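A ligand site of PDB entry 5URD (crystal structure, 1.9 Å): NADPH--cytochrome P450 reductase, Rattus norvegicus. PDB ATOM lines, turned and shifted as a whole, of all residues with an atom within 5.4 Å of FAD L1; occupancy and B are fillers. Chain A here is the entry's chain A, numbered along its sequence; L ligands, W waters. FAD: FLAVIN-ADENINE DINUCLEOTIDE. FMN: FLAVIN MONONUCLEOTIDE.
The side-chain hydroxyl (OG1) of Thr 435 lies within hydrogen-bond range of the backbone NH (N) of Val 420 (3.0 Å). The backbone NH (N) of Gly 432 is in hydrogen-bond range of the backbone carbonyl oxygen (O) of Val 420 (2.8 Å). O of Gly 432 sits at hydrogen-bond distance from OG of Ser 436, at 2.7 Å. A ring nitrogen (NE2) of His 263 sits at hydrogen-bond distance from the side-chain carboxylate (OD1) of Asp 619, 2.8 Å away. The side-chain carboxylate (OD2) of Asp 619 is in hydrogen-bond range of the side-chain hydroxyl (OG) of Ser 401, at 2.8 Å. The guanidinium group of Arg 368 sits at hydrogen-bond distance from the side-chain amide oxygen of Asn 323, at 3.1 Å. The guanidinium group of Arg 368 sits at hydrogen-bond distance from the side-chain hydroxyl of Tyr 422, 3.2 Å away.
Water W9 bridges O2' of FAD L1 (2.6 Å) and N of Tyr 399 (3.1 Å). Water W12 lies within hydrogen-bond range of OG1 of Thr 322 (2.6 Å), O1A of FAD L1 (2.7 Å) and OD1 of Asn 323 (2.8 Å). Water W2 lies within hydrogen-bond range of the side-chain hydroxyl of Tyr 422, an oxygen (O4B) of FAD L1 and the guanidinium group of Arg 368. Water W8 lies within hydrogen-bond range of the backbone carbonyl oxygen of Ser 401 (2.7 Å), an oxygen (O4) of FAD L1 (2.8 Å) and the backbone NH of Cys 416 (2.8 Å). Water W13 lies within hydrogen-bond range of the backbone carbonyl oxygen of Lys 431 and an oxygen (O1A) of FAD L1. Water W6 lies within hydrogen-bond range of the indole nitrogen of Trp 621, the side-chain hydroxyl of Thr 479 and a nitrogen (N1) of FAD L1.
NE1 of Trp 621 lies close to N10 of FAD L1, at 3.5 Å. NE2 of His 263 touches C7M of FAD L1, 3.6 Å away. CA of Ala 417 touches O2 of FAD L1, at 3.2 Å. Val 420 touches FAD L1 (CG2 to C5', 3.9 Å). Tyr 422 touches FAD L1. Gly 432 touches FAD L1. Ala 482 touches FAD L1. 17 residues have an atom within 4 Å of FAD L1: His 263, Arg 368, Arg 398, Tyr 399, Tyr 400, Ser 401, Cys 416, Ala 417, Val 418, Val 420, Tyr 422, Gly 432, Val 433, Ala 434, Thr 435, Ala 482 and Trp 621. The nearest printed residue that does not touch FAD L1 is Thr 479 (4.04 Å).
An oxygen (O2P) of FAD L1 is in hydrogen-bond range of the backbone NH (N) of Ala 434, at 2.8 Å. The guanidinium group (NH2) of Arg 368 lies within hydrogen-bond range of an oxygen (O2B) of FAD L1, at 3.0 Å. An oxygen (O4) of FAD L1 lies within hydrogen-bond range of the backbone NH (N) of Ser 401, at 3.0 Å. N of Thr 435 lies within hydrogen-bond range of O1P of FAD L1, 2.9 Å away. The side-chain hydroxyl (OG1) of Thr 435 sits at hydrogen-bond distance from an oxygen (O1P) of FAD L1, at 2.7 Å. O of Cys 416 lies within hydrogen-bond range of N3 of FAD L1 (2.8 Å). The backbone NH (N) of Tyr 399 lies within hydrogen-bond range of an oxygen (O2') of FAD L1. The side-chain hydroxyl of Tyr 400 is in hydrogen-bond range of an oxygen (O4') of FAD L1 (2.7 Å). N of Val 433 sits at hydrogen-bond distance from O1A of FAD L1. An oxygen (O2') of FAD L1 is in hydrogen-bond range of the backbone carbonyl oxygen (O) of Tyr 399, 2.6 Å away. OG of Ser 401 is in hydrogen-bond range of N5 of FAD L1 (3.4 Å). An oxygen (O2) of FAD L1 lies within hydrogen-bond range of the backbone NH of Val 418 (3.2 Å). The guanidinium group (NE) of Arg 398 lies within salt-bridge range of an oxygen (O2P) of FAD L1, 2.8 Å away.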
ATOM      1  N   HIS A 263     -16.835 -24.150 -19.297  1.00  0.00           N
ATOM      2  CA  HIS A 263     -18.043 -23.500 -19.771  1.00  0.00           C
ATOM      3  C   HIS A 263     -19.093 -23.490 -18.683  1.00  0.00           C
ATOM      4  O   HIS A 263     -19.118 -24.383 -17.829  1.00  0.00           O
ATOM      5  CB  HIS A 263     -18.603 -24.235 -20.998  1.00  0.00           C
ATOM      6  CG  HIS A 263     -17.695 -24.225 -22.193  1.00  0.00           C
ATOM      7  ND1 HIS A 263     -17.120 -25.371 -22.697  1.00  0.00           N
ATOM      8  CD2 HIS A 263     -17.272 -23.211 -22.987  1.00  0.00           C
ATOM      9  CE1 HIS A 263     -16.394 -25.065 -23.753  1.00  0.00           C
ATOM     10  NE2 HIS A 263     -16.463 -23.757 -23.951  1.00  0.00           N
ATOM     11  N   THR A 322     -38.928 -20.882 -30.101  1.00  0.00           N
ATOM     12  CA  THR A 322     -38.339 -19.850 -30.939  1.00  0.00           C
ATOM     13  C   THR A 322     -37.612 -20.302 -32.196  1.00  0.00           C
ATOM     14  O   THR A 322     -37.521 -19.538 -33.141  1.00  0.00           O
ATOM     15  CB  THR A 322     -37.374 -19.009 -30.109  1.00  0.00           C
ATOM     16  OG1 THR A 322     -36.476 -19.876 -29.416  1.00  0.00           O
ATOM     17  CG2 THR A 322     -38.138 -18.163 -29.073  1.00  0.00           C
ATOM     18  N   ASN A 323     -37.085 -21.520 -32.201  1.00  0.00           N
ATOM     19  CA  ASN A 323     -36.392 -21.973 -33.402  1.00  0.00           C
ATOM     20  C   ASN A 323     -37.375 -22.506 -34.449  1.00  0.00           C
ATOM     21  O   ASN A 323     -38.463 -22.959 -34.111  1.00  0.00           O
ATOM     22  CB  ASN A 323     -35.369 -23.059 -33.046  1.00  0.00           C
ATOM     23  CG  ASN A 323     -34.199 -22.518 -32.246  1.00  0.00           C
ATOM     24  OD1 ASN A 323     -33.646 -21.459 -32.570  1.00  0.00           O
ATOM     25  ND2 ASN A 323     -33.817 -23.227 -31.194  1.00  0.00           N
ATOM     26  N   ARG A 368     -36.634 -17.628 -40.558  1.00  0.00           N
ATOM     27  CA  ARG A 368     -36.572 -17.851 -39.104  1.00  0.00           C
ATOM     28  C   ARG A 368     -37.944 -17.715 -38.437  1.00  0.00           C
ATOM     29  O   ARG A 368     -38.085 -17.059 -37.401  1.00  0.00           O
ATOM     30  CB  ARG A 368     -35.570 -16.879 -38.447  1.00  0.00           C
ATOM     31  CG  ARG A 368     -34.107 -17.089 -38.857  1.00  0.00           C
ATOM     32  CD  ARG A 368     -33.534 -18.392 -38.297  1.00  0.00           C
ATOM     33  NE  ARG A 368     -33.580 -18.426 -36.831  1.00  0.00           N
ATOM     34  CZ  ARG A 368     -33.115 -19.419 -36.083  1.00  0.00           C
ATOM     35  NH1 ARG A 368     -33.198 -19.356 -34.764  1.00  0.00           N
ATOM     36  NH2 ARG A 368     -32.557 -20.483 -36.657  1.00  0.00           N
ATOM     37  N   ARG A 398     -27.911 -23.028 -22.499  1.00  0.00           N
ATOM     38  CA  ARG A 398     -26.980 -22.324 -23.368  1.00  0.00           C
ATOM     39  C   ARG A 398     -25.624 -22.286 -22.666  1.00  0.00           C
ATOM     40  O   ARG A 398     -25.550 -22.053 -21.461  1.00  0.00           O
ATOM     41  CB  ARG A 398     -27.446 -20.888 -23.653  1.00  0.00           C
ATOM     42  CG  ARG A 398     -28.332 -20.712 -24.899  1.00  0.00           C
ATOM     43  CD  ARG A 398     -29.688 -21.399 -24.780  1.00  0.00           C
ATOM     44  NE  ARG A 398     -30.590 -20.950 -25.848  1.00  0.00           N
ATOM     45  CZ  ARG A 398     -31.711 -21.571 -26.202  1.00  0.00           C
ATOM     46  NH1 ARG A 398     -32.454 -21.066 -27.183  1.00  0.00           N
ATOM     47  NH2 ARG A 398     -32.100 -22.673 -25.588  1.00  0.00           N
ATOM     48  N   TYR A 399     -24.571 -22.511 -23.432  1.00  0.00           N
ATOM     49  CA  TYR A 399     -23.198 -22.498 -22.904  1.00  0.00           C
ATOM     50  C   TYR A 399     -22.482 -21.178 -23.148  1.00  0.00           C
ATOM     51  O   TYR A 399     -22.643 -20.549 -24.197  1.00  0.00           O
ATOM     52  CB  TYR A 399     -22.392 -23.631 -23.540  1.00  0.00           C
ATOM     53  CG  TYR A 399     -22.846 -24.998 -23.120  1.00  0.00           C
ATOM     54  CD1 TYR A 399     -22.459 -25.533 -21.901  1.00  0.00           C
ATOM     55  CD2 TYR A 399     -23.715 -25.741 -23.926  1.00  0.00           C
ATOM     56  CE1 TYR A 399     -22.926 -26.780 -21.475  1.00  0.00           C
ATOM     57  CE2 TYR A 399     -24.181 -26.995 -23.508  1.00  0.00           C
ATOM     58  CZ  TYR A 399     -23.787 -27.503 -22.287  1.00  0.00           C
ATOM     59  OH  TYR A 399     -24.242 -28.732 -21.851  1.00  0.00           O
ATOM     60  N   TYR A 400     -21.675 -20.786 -22.176  1.00  0.00           N
ATOM     61  CA  TYR A 400     -20.877 -19.563 -22.242  1.00  0.00           C
ATOM     62  C   TYR A 400     -19.482 -19.883 -21.727  1.00  0.00           C
ATOM     63  O   TYR A 400     -19.320 -20.668 -20.792  1.00  0.00           O
ATOM     64  CB  TYR A 400     -21.536 -18.463 -21.411  1.00  0.00           C
ATOM     65  CG  TYR A 400     -22.863 -18.046 -22.003  1.00  0.00           C
ATOM     66  CD1 TYR A 400     -22.907 -17.153 -23.080  1.00  0.00           C
ATOM     67  CD2 TYR A 400     -24.052 -18.631 -21.583  1.00  0.00           C
ATOM     68  CE1 TYR A 400     -24.107 -16.868 -23.724  1.00  0.00           C
ATOM     69  CE2 TYR A 400     -25.257 -18.353 -22.221  1.00  0.00           C
ATOM     70  CZ  TYR A 400     -25.277 -17.481 -23.288  1.00  0.00           C
ATOM     71  OH  TYR A 400     -26.441 -17.248 -23.976  1.00  0.00           O
ATOM     72  N   SER A 401     -18.469 -19.308 -22.356  1.00  0.00           N
ATOM     73  CA  SER A 401     -17.090 -19.546 -21.942  1.00  0.00           C
ATOM     74  C   SER A 401     -16.837 -18.734 -20.667  1.00  0.00           C
ATOM     75  O   SER A 401     -16.884 -17.507 -20.694  1.00  0.00           O
ATOM     76  CB  SER A 401     -16.129 -19.094 -23.038  1.00  0.00           C
ATOM     77  OG  SER A 401     -16.431 -19.742 -24.271  1.00  0.00           O
ATOM     78  N   CYS A 416     -19.390 -13.289 -20.606  1.00  0.00           N
ATOM     79  CA  CYS A 416     -19.248 -12.216 -21.576  1.00  0.00           C
ATOM     80  C   CYS A 416     -20.108 -12.649 -22.755  1.00  0.00           C
ATOM     81  O   CYS A 416     -19.790 -13.640 -23.430  1.00  0.00           O
ATOM     82  CB  CYS A 416     -17.794 -12.078 -22.027  1.00  0.00           C
ATOM     83  SG  CYS A 416     -17.518 -10.979 -23.439  1.00  0.00           S
ATOM     84  N   ALA A 417     -21.197 -11.946 -23.013  1.00  0.00           N
ATOM     85  CA  ALA A 417     -22.084 -12.355 -24.106  1.00  0.00           C
ATOM     86  C   ALA A 417     -22.675 -11.203 -24.900  1.00  0.00           C
ATOM     87  O   ALA A 417     -22.853 -10.095 -24.390  1.00  0.00           O
ATOM     88  CB  ALA A 417     -23.201 -13.207 -23.549  1.00  0.00           C
ATOM     89  N   VAL A 418     -22.969 -11.479 -26.170  1.00  0.00           N
ATOM     90  CA  VAL A 418     -23.602 -10.475 -27.019  1.00  0.00           C
ATOM     91  C   VAL A 418     -25.089 -10.804 -27.077  1.00  0.00           C
ATOM     92  O   VAL A 418     -25.474 -11.958 -27.313  1.00  0.00           O
ATOM     93  CB  VAL A 418     -22.975 -10.446 -28.448  1.00  0.00           C
ATOM     94  CG1 VAL A 418     -23.003 -11.831 -29.084  1.00  0.00           C
ATOM     95  CG2 VAL A 418     -23.710  -9.443 -29.320  1.00  0.00           C
ATOM     96  N   VAL A 420     -28.633 -11.301 -28.496  1.00  0.00           N
ATOM     97  CA  VAL A 420     -29.123 -11.640 -29.820  1.00  0.00           C
ATOM     98  C   VAL A 420     -30.466 -10.974 -30.051  1.00  0.00           C
ATOM     99  O   VAL A 420     -31.405 -11.181 -29.290  1.00  0.00           O
ATOM    100  CB  VAL A 420     -29.273 -13.172 -29.989  1.00  0.00           C
ATOM    101  CG1 VAL A 420     -29.915 -13.499 -31.341  1.00  0.00           C
ATOM    102  CG2 VAL A 420     -27.917 -13.826 -29.898  1.00  0.00           C
ATOM    103  N   TYR A 422     -32.424  -9.537 -33.804  1.00  0.00           N
ATOM    104  CA  TYR A 422     -32.286  -9.228 -35.225  1.00  0.00           C
ATOM    105  C   TYR A 422     -33.616  -9.242 -35.950  1.00  0.00           C
ATOM    106  O   TYR A 422     -34.559  -9.891 -35.526  1.00  0.00           O
ATOM    107  CB  TYR A 422     -31.370 -10.249 -35.894  1.00  0.00           C
ATOM    108  CG  TYR A 422     -31.872 -11.675 -35.792  1.00  0.00           C
ATOM    109  CD1 TYR A 422     -31.680 -12.421 -34.621  1.00  0.00           C
ATOM    110  CD2 TYR A 422     -32.587 -12.270 -36.834  1.00  0.00           C
ATOM    111  CE1 TYR A 422     -32.188 -13.715 -34.496  1.00  0.00           C
ATOM    112  CE2 TYR A 422     -33.104 -13.561 -36.712  1.00  0.00           C
ATOM    113  CZ  TYR A 422     -32.905 -14.273 -35.533  1.00  0.00           C
ATOM    114  OH  TYR A 422     -33.452 -15.529 -35.394  1.00  0.00           O
ATOM    115  N   LYS A 431     -35.638 -12.495 -30.832  1.00  0.00           N
ATOM    116  CA  LYS A 431     -34.783 -12.234 -29.677  1.00  0.00           C
ATOM    117  C   LYS A 431     -34.171 -13.543 -29.193  1.00  0.00           C
ATOM    118  O   LYS A 431     -34.868 -14.546 -29.084  1.00  0.00           O
ATOM    119  CB  LYS A 431     -35.626 -11.652 -28.538  1.00  0.00           C
ATOM    120  CG  LYS A 431     -36.452 -10.425 -28.902  1.00  0.00           C
ATOM    121  CD  LYS A 431     -35.592  -9.188 -28.976  1.00  0.00           C
ATOM    122  CE  LYS A 431     -34.957  -8.881 -27.618  1.00  0.00           C
ATOM    123  NZ  LYS A 431     -35.994  -8.785 -26.560  1.00  0.00           N
ATOM    124  N   GLY A 432     -32.877 -13.527 -28.890  1.00  0.00           N
ATOM    125  CA  GLY A 432     -32.228 -14.729 -28.396  1.00  0.00           C
ATOM    126  C   GLY A 432     -32.845 -15.071 -27.048  1.00  0.00           C
ATOM    127  O   GLY A 432     -33.031 -14.197 -26.197  1.00  0.00           O
ATOM    128  N   VAL A 433     -33.159 -16.346 -26.836  1.00  0.00           N
ATOM    129  CA  VAL A 433     -33.774 -16.751 -25.567  1.00  0.00           C
ATOM    130  C   VAL A 433     -32.917 -16.494 -24.335  1.00  0.00           C
ATOM    131  O   VAL A 433     -33.302 -15.747 -23.432  1.00  0.00           O
ATOM    132  CB  VAL A 433     -34.178 -18.246 -25.598  1.00  0.00           C
ATOM    133  CG1 VAL A 433     -34.785 -18.655 -24.265  1.00  0.00           C
ATOM    134  CG2 VAL A 433     -35.186 -18.512 -26.734  1.00  0.00           C
ATOM    135  N   ALA A 434     -31.743 -17.100 -24.284  1.00  0.00           N
ATOM    136  CA  ALA A 434     -30.872 -16.938 -23.126  1.00  0.00           C
ATOM    137  C   ALA A 434     -30.320 -15.519 -22.930  1.00  0.00           C
ATOM    138  O   ALA A 434     -30.307 -15.010 -21.799  1.00  0.00           O
ATOM    139  CB  ALA A 434     -29.721 -17.941 -23.186  1.00  0.00           C
ATOM    140  N   THR A 435     -29.880 -14.882 -24.011  1.00  0.00           N
ATOM    141  CA  THR A 435     -29.313 -13.544 -23.858  1.00  0.00           C
ATOM    142  C   THR A 435     -30.344 -12.487 -23.468  1.00  0.00           C
ATOM    143  O   THR A 435     -30.036 -11.583 -22.698  1.00  0.00           O
ATOM    144  CB  THR A 435     -28.516 -13.114 -25.121  1.00  0.00           C
ATOM    145  OG1 THR A 435     -29.348 -13.183 -26.283  1.00  0.00           O
ATOM    146  CG2 THR A 435     -27.290 -14.028 -25.308  1.00  0.00           C
ATOM    147  N   SER A 436     -31.572 -12.590 -23.976  1.00  0.00           N
ATOM    148  CA  SER A 436     -32.615 -11.609 -23.610  1.00  0.00           C
ATOM    149  C   SER A 436     -32.942 -11.791 -22.123  1.00  0.00           C
ATOM    150  O   SER A 436     -33.145 -10.819 -21.388  1.00  0.00           O
ATOM    151  CB  SER A 436     -33.892 -11.830 -24.419  1.00  0.00           C
ATOM    152  OG  SER A 436     -33.685 -11.570 -25.797  1.00  0.00           O
ATOM    153  N   THR A 479     -16.644 -11.629 -28.940  1.00  0.00           N
ATOM    154  CA  THR A 479     -16.903 -12.365 -27.712  1.00  0.00           C
ATOM    155  C   THR A 479     -15.932 -13.531 -27.537  1.00  0.00           C
ATOM    156  O   THR A 479     -15.975 -14.230 -26.525  1.00  0.00           O
ATOM    157  CB  THR A 479     -18.358 -12.892 -27.651  1.00  0.00           C
ATOM    158  OG1 THR A 479     -18.622 -13.738 -28.778  1.00  0.00           O
ATOM    159  CG2 THR A 479     -19.349 -11.723 -27.629  1.00  0.00           C
ATOM    160  N   ALA A 482     -13.796 -13.856 -24.274  1.00  0.00           N
ATOM    161  CA  ALA A 482     -14.309 -14.432 -23.019  1.00  0.00           C
ATOM    162  C   ALA A 482     -13.367 -15.289 -22.175  1.00  0.00           C
ATOM    163  O   ALA A 482     -13.004 -14.899 -21.059  1.00  0.00           O
ATOM    164  CB  ALA A 482     -15.621 -15.183 -23.288  1.00  0.00           C
ATOM    165  N   ASP A 619     -12.001 -23.195 -29.092  1.00  0.00           N
ATOM    166  CA  ASP A 619     -13.220 -22.978 -28.334  1.00  0.00           C
ATOM    167  C   ASP A 619     -14.020 -22.066 -29.249  1.00  0.00           C
ATOM    168  O   ASP A 619     -14.140 -20.870 -29.023  1.00  0.00           O
ATOM    169  CB  ASP A 619     -12.945 -22.270 -26.993  1.00  0.00           C
ATOM    170  CG  ASP A 619     -14.219 -22.056 -26.180  1.00  0.00           C
ATOM    171  OD1 ASP A 619     -15.165 -22.858 -26.317  1.00  0.00           O
ATOM    172  OD2 ASP A 619     -14.276 -21.081 -25.391  1.00  0.00           O
ATOM    173  N   VAL A 620     -14.532 -22.661 -30.328  1.00  0.00           N
ATOM    174  CA  VAL A 620     -15.305 -21.899 -31.302  1.00  0.00           C
ATOM    175  C   VAL A 620     -16.735 -22.395 -31.400  1.00  0.00           C
ATOM    176  O   VAL A 620     -17.038 -23.553 -31.106  1.00  0.00           O
ATOM    177  CB  VAL A 620     -14.646 -21.953 -32.701  1.00  0.00           C
ATOM    178  CG1 VAL A 620     -13.306 -21.233 -32.669  1.00  0.00           C
ATOM    179  CG2 VAL A 620     -14.444 -23.393 -33.142  1.00  0.00           C
ATOM    180  N   TRP A 621     -17.625 -21.508 -31.811  1.00  0.00           N
ATOM    181  CA  TRP A 621     -19.029 -21.834 -31.937  1.00  0.00           C
ATOM    182  C   TRP A 621     -19.645 -20.976 -33.022  1.00  0.00           C
ATOM    183  O   TRP A 621     -19.045 -20.010 -33.476  1.00  0.00           O
ATOM    184  CB  TRP A 621     -19.747 -21.608 -30.607  1.00  0.00           C
ATOM    185  CG  TRP A 621     -19.771 -20.155 -30.159  1.00  0.00           C
ATOM    186  CD1 TRP A 621     -20.700 -19.204 -30.482  1.00  0.00           C
ATOM    187  CD2 TRP A 621     -18.802 -19.504 -29.334  1.00  0.00           C
ATOM    188  NE1 TRP A 621     -20.362 -17.997 -29.918  1.00  0.00           N
ATOM    189  CE2 TRP A 621     -19.195 -18.152 -29.210  1.00  0.00           C
ATOM    190  CE3 TRP A 621     -17.625 -19.915 -28.693  1.00  0.00           C
ATOM    191  CZ2 TRP A 621     -18.467 -17.208 -28.465  1.00  0.00           C
ATOM    192  CZ3 TRP A 621     -16.901 -18.985 -27.950  1.00  0.00           C
ATOM    193  CH2 TRP A 621     -17.323 -17.645 -27.843  1.00  0.00           C
ATOM    194  N   SER A 622     -20.863 -21.328 -33.418  1.00  0.00           N
ATOM    195  CA  SER A 622     -21.584 -20.599 -34.439  1.00  0.00           C
ATOM    196  C   SER A 622     -23.076 -20.796 -34.218  1.00  0.00           C
ATOM    197  O   SER A 622     -23.809 -19.782 -34.198  1.00  0.00           O
ATOM    198  CB  SER A 622     -21.177 -21.101 -35.821  1.00  0.00           C
ATOM    199  OG  SER A 622     -21.204 -22.517 -35.880  1.00  0.00           O
ATOM    200  OXT SER A 622     -23.490 -21.962 -34.071  1.00  0.00           O
HETATM  201  PA  FAD L   1     -31.097 -18.316 -29.429  1.00  0.00           P
HETATM  202  O1A FAD L   1     -32.528 -18.074 -29.107  1.00  0.00           O
HETATM  203  O2A FAD L   1     -30.507 -19.625 -29.119  1.00  0.00           O
HETATM  204  O5B FAD L   1     -30.886 -17.976 -30.990  1.00  0.00           O
HETATM  205  C5B FAD L   1     -29.665 -18.330 -31.650  1.00  0.00           C
HETATM  206  C4B FAD L   1     -29.938 -18.408 -33.147  1.00  0.00           C
HETATM  207  O4B FAD L   1     -30.376 -17.143 -33.655  1.00  0.00           O
HETATM  208  C3B FAD L   1     -28.643 -18.615 -33.922  1.00  0.00           C
HETATM  209  O3B FAD L   1     -28.278 -20.001 -33.829  1.00  0.00           O
HETATM  210  C2B FAD L   1     -29.177 -18.339 -35.321  1.00  0.00           C
HETATM  211  O2B FAD L   1     -29.885 -19.491 -35.807  1.00  0.00           O
HETATM  212  C1B FAD L   1     -30.160 -17.191 -35.076  1.00  0.00           C
HETATM  213  N9A FAD L   1     -29.591 -15.885 -35.466  1.00  0.00           N
HETATM  214  C8A FAD L   1     -28.673 -15.059 -34.668  1.00  0.00           C
HETATM  215  N7A FAD L   1     -28.537 -13.879 -35.546  1.00  0.00           N
HETATM  216  C5A FAD L   1     -29.230 -14.096 -36.658  1.00  0.00           C
HETATM  217  C6A FAD L   1     -29.375 -13.309 -37.722  1.00  0.00           C
HETATM  218  N6A FAD L   1     -28.818 -12.111 -37.643  1.00  0.00           N
HETATM  219  N1A FAD L   1     -30.044 -13.694 -38.817  1.00  0.00           N
HETATM  220  C2A FAD L   1     -30.587 -14.985 -38.857  1.00  0.00           C
HETATM  221  N3A FAD L   1     -30.416 -15.789 -37.729  1.00  0.00           N
HETATM  222  C4A FAD L   1     -29.746 -15.329 -36.668  1.00  0.00           C
HETATM  223  N1  FAD L   1     -21.926 -16.804 -26.794  1.00  0.00           N
HETATM  224  C2  FAD L   1     -21.456 -15.633 -26.195  1.00  0.00           C
HETATM  225  O2  FAD L   1     -21.974 -14.557 -26.460  1.00  0.00           O
HETATM  226  N3  FAD L   1     -20.364 -15.698 -25.314  1.00  0.00           N
HETATM  227  C4  FAD L   1     -19.741 -16.924 -25.056  1.00  0.00           C
HETATM  228  O4  FAD L   1     -18.856 -16.970 -24.200  1.00  0.00           O
HETATM  229  C4X FAD L   1     -20.198 -18.083 -25.681  1.00  0.00           C
HETATM  230  N5  FAD L   1     -19.510 -19.225 -25.561  1.00  0.00           N
HETATM  231  C5X FAD L   1     -19.956 -20.344 -26.154  1.00  0.00           C
HETATM  232  C6  FAD L   1     -19.270 -21.546 -25.987  1.00  0.00           C
HETATM  233  C7  FAD L   1     -19.759 -22.713 -26.563  1.00  0.00           C
HETATM  234  C7M FAD L   1     -19.064 -23.902 -26.408  1.00  0.00           C
HETATM  235  C8  FAD L   1     -20.930 -22.672 -27.314  1.00  0.00           C
HETATM  236  C8M FAD L   1     -21.438 -23.843 -27.874  1.00  0.00           C
HETATM  237  C9  FAD L   1     -21.625 -21.483 -27.469  1.00  0.00           C
HETATM  238  C9A FAD L   1     -21.141 -20.315 -26.879  1.00  0.00           C
HETATM  239  N10 FAD L   1     -21.830 -19.166 -26.992  1.00  0.00           N
HETATM  240  C10 FAD L   1     -21.277 -18.023 -26.542  1.00  0.00           C
HETATM  241  C1' FAD L   1     -23.108 -19.091 -27.731  1.00  0.00           C
HETATM  242  C2' FAD L   1     -24.274 -19.236 -26.741  1.00  0.00           C
HETATM  243  O2' FAD L   1     -24.277 -20.565 -26.198  1.00  0.00           O
HETATM  244  C3' FAD L   1     -25.629 -18.969 -27.396  1.00  0.00           C
HETATM  245  O3' FAD L   1     -25.728 -19.700 -28.610  1.00  0.00           O
HETATM  246  C4' FAD L   1     -25.816 -17.472 -27.700  1.00  0.00           C
HETATM  247  O4' FAD L   1     -25.651 -16.715 -26.493  1.00  0.00           O
HETATM  248  C5' FAD L   1     -27.221 -17.249 -28.259  1.00  0.00           C
HETATM  249  O5' FAD L   1     -28.183 -17.844 -27.376  1.00  0.00           O
HETATM  250  P   FAD L   1     -29.668 -17.242 -27.226  1.00  0.00           P
HETATM  251  O1P FAD L   1     -29.573 -15.851 -26.731  1.00  0.00           O
HETATM  252  O2P FAD L   1     -30.469 -18.222 -26.462  1.00  0.00           O
HETATM  253  O3P FAD L   1     -30.188 -17.175 -28.754  1.00  0.00           O
HETATM  254  N1  FMN L   2     -19.510 -31.402 -35.678  1.00  0.00           N
HETATM  255  C2  FMN L   2     -18.552 -32.161 -36.237  1.00  0.00           C
HETATM  256  O2  FMN L   2     -18.749 -32.780 -37.288  1.00  0.00           O
HETATM  257  N3  FMN L   2     -17.341 -32.223 -35.576  1.00  0.00           N
HETATM  258  C4  FMN L   2     -16.989 -31.571 -34.386  1.00  0.00           C
HETATM  259  O4  FMN L   2     -15.848 -31.783 -33.994  1.00  0.00           O
HETATM  260  C4A FMN L   2     -17.979 -30.754 -33.788  1.00  0.00           C
HETATM  261  N5  FMN L   2     -17.652 -30.074 -32.600  1.00  0.00           N
HETATM  262  C5A FMN L   2     -18.682 -29.279 -32.085  1.00  0.00           C
HETATM  263  C6  FMN L   2     -18.372 -28.558 -30.882  1.00  0.00           C
HETATM  264  C7  FMN L   2     -19.316 -27.703 -30.262  1.00  0.00           C
HETATM  265  C7M FMN L   2     -18.841 -26.993 -28.975  1.00  0.00           C
HETATM  266  C8  FMN L   2     -20.681 -27.533 -30.849  1.00  0.00           C
HETATM  267  C8M FMN L   2     -21.693 -26.734 -30.349  1.00  0.00           C
HETATM  268  C9  FMN L   2     -20.999 -28.224 -32.010  1.00  0.00           C
HETATM  269  C9A FMN L   2     -20.025 -29.107 -32.671  1.00  0.00           C
HETATM  270  N10 FMN L   2     -20.296 -29.864 -33.918  1.00  0.00           N
HETATM  271  C10 FMN L   2     -19.241 -30.713 -34.505  1.00  0.00           C
HETATM  272  C1' FMN L   2     -21.604 -29.771 -34.563  1.00  0.00           C
HETATM  273  C2' FMN L   2     -22.661 -30.784 -34.021  1.00  0.00           C
HETATM  274  O2' FMN L   2     -22.152 -32.171 -34.214  1.00  0.00           O
HETATM  275  C3' FMN L   2     -23.991 -30.594 -34.740  1.00  0.00           C
HETATM  276  O3' FMN L   2     -24.437 -29.242 -34.477  1.00  0.00           O
HETATM  277  C4' FMN L   2     -25.022 -31.658 -34.187  1.00  0.00           C
HETATM  278  O4' FMN L   2     -26.197 -31.327 -35.004  1.00  0.00           O
HETATM  279  C5' FMN L   2     -25.455 -31.453 -32.748  1.00  0.00           C
HETATM  280  O5' FMN L   2     -26.393 -32.521 -32.296  1.00  0.00           O
HETATM  281  P   FMN L   2     -27.091 -32.626 -30.882  1.00  0.00           P
HETATM  282  O1P FMN L   2     -28.056 -31.492 -30.751  1.00  0.00           O
HETATM  283  O2P FMN L   2     -25.909 -32.749 -29.875  1.00  0.00           O
HETATM  284  O3P FMN L   2     -27.921 -33.991 -31.034  1.00  0.00           O
HETATM  285  O   HOH W   1     -24.166 -22.259 -30.048  1.00  0.00           O
HETATM  286  O   HOH W   2     -33.101 -16.876 -33.147  1.00  0.00           O
HETATM  287  O   HOH W   3     -24.425 -14.534 -27.552  1.00  0.00           O
HETATM  288  O   HOH W   4     -30.080 -10.024 -39.465  1.00  0.00           O
HETATM  289  O   HOH W   5     -30.220 -22.390 -33.074  1.00  0.00           O
HETATM  290  O   HOH W   6     -21.036 -15.303 -29.733  1.00  0.00           O
HETATM  291  O   HOH W   7     -27.109 -11.952 -34.531  1.00  0.00           O
HETATM  292  O   HOH W   8     -18.769 -15.870 -21.602  1.00  0.00           O
HETATM  293  O   HOH W   9     -25.187 -23.040 -26.398  1.00  0.00           O
HETATM  294  O   HOH W  10     -25.495 -18.933 -31.179  1.00  0.00           O
HETATM  295  O   HOH W  11     -28.199 -21.032 -28.849  1.00  0.00           O
HETATM  296  O   HOH W  12     -34.065 -19.857 -30.366  1.00  0.00           O
HETATM  297  O   HOH W  13     -34.636 -16.600 -30.960  1.00  0.00           O
HETATM  298  O   HOH W  14     -31.011 -22.043 -30.325  1.00  0.00           O
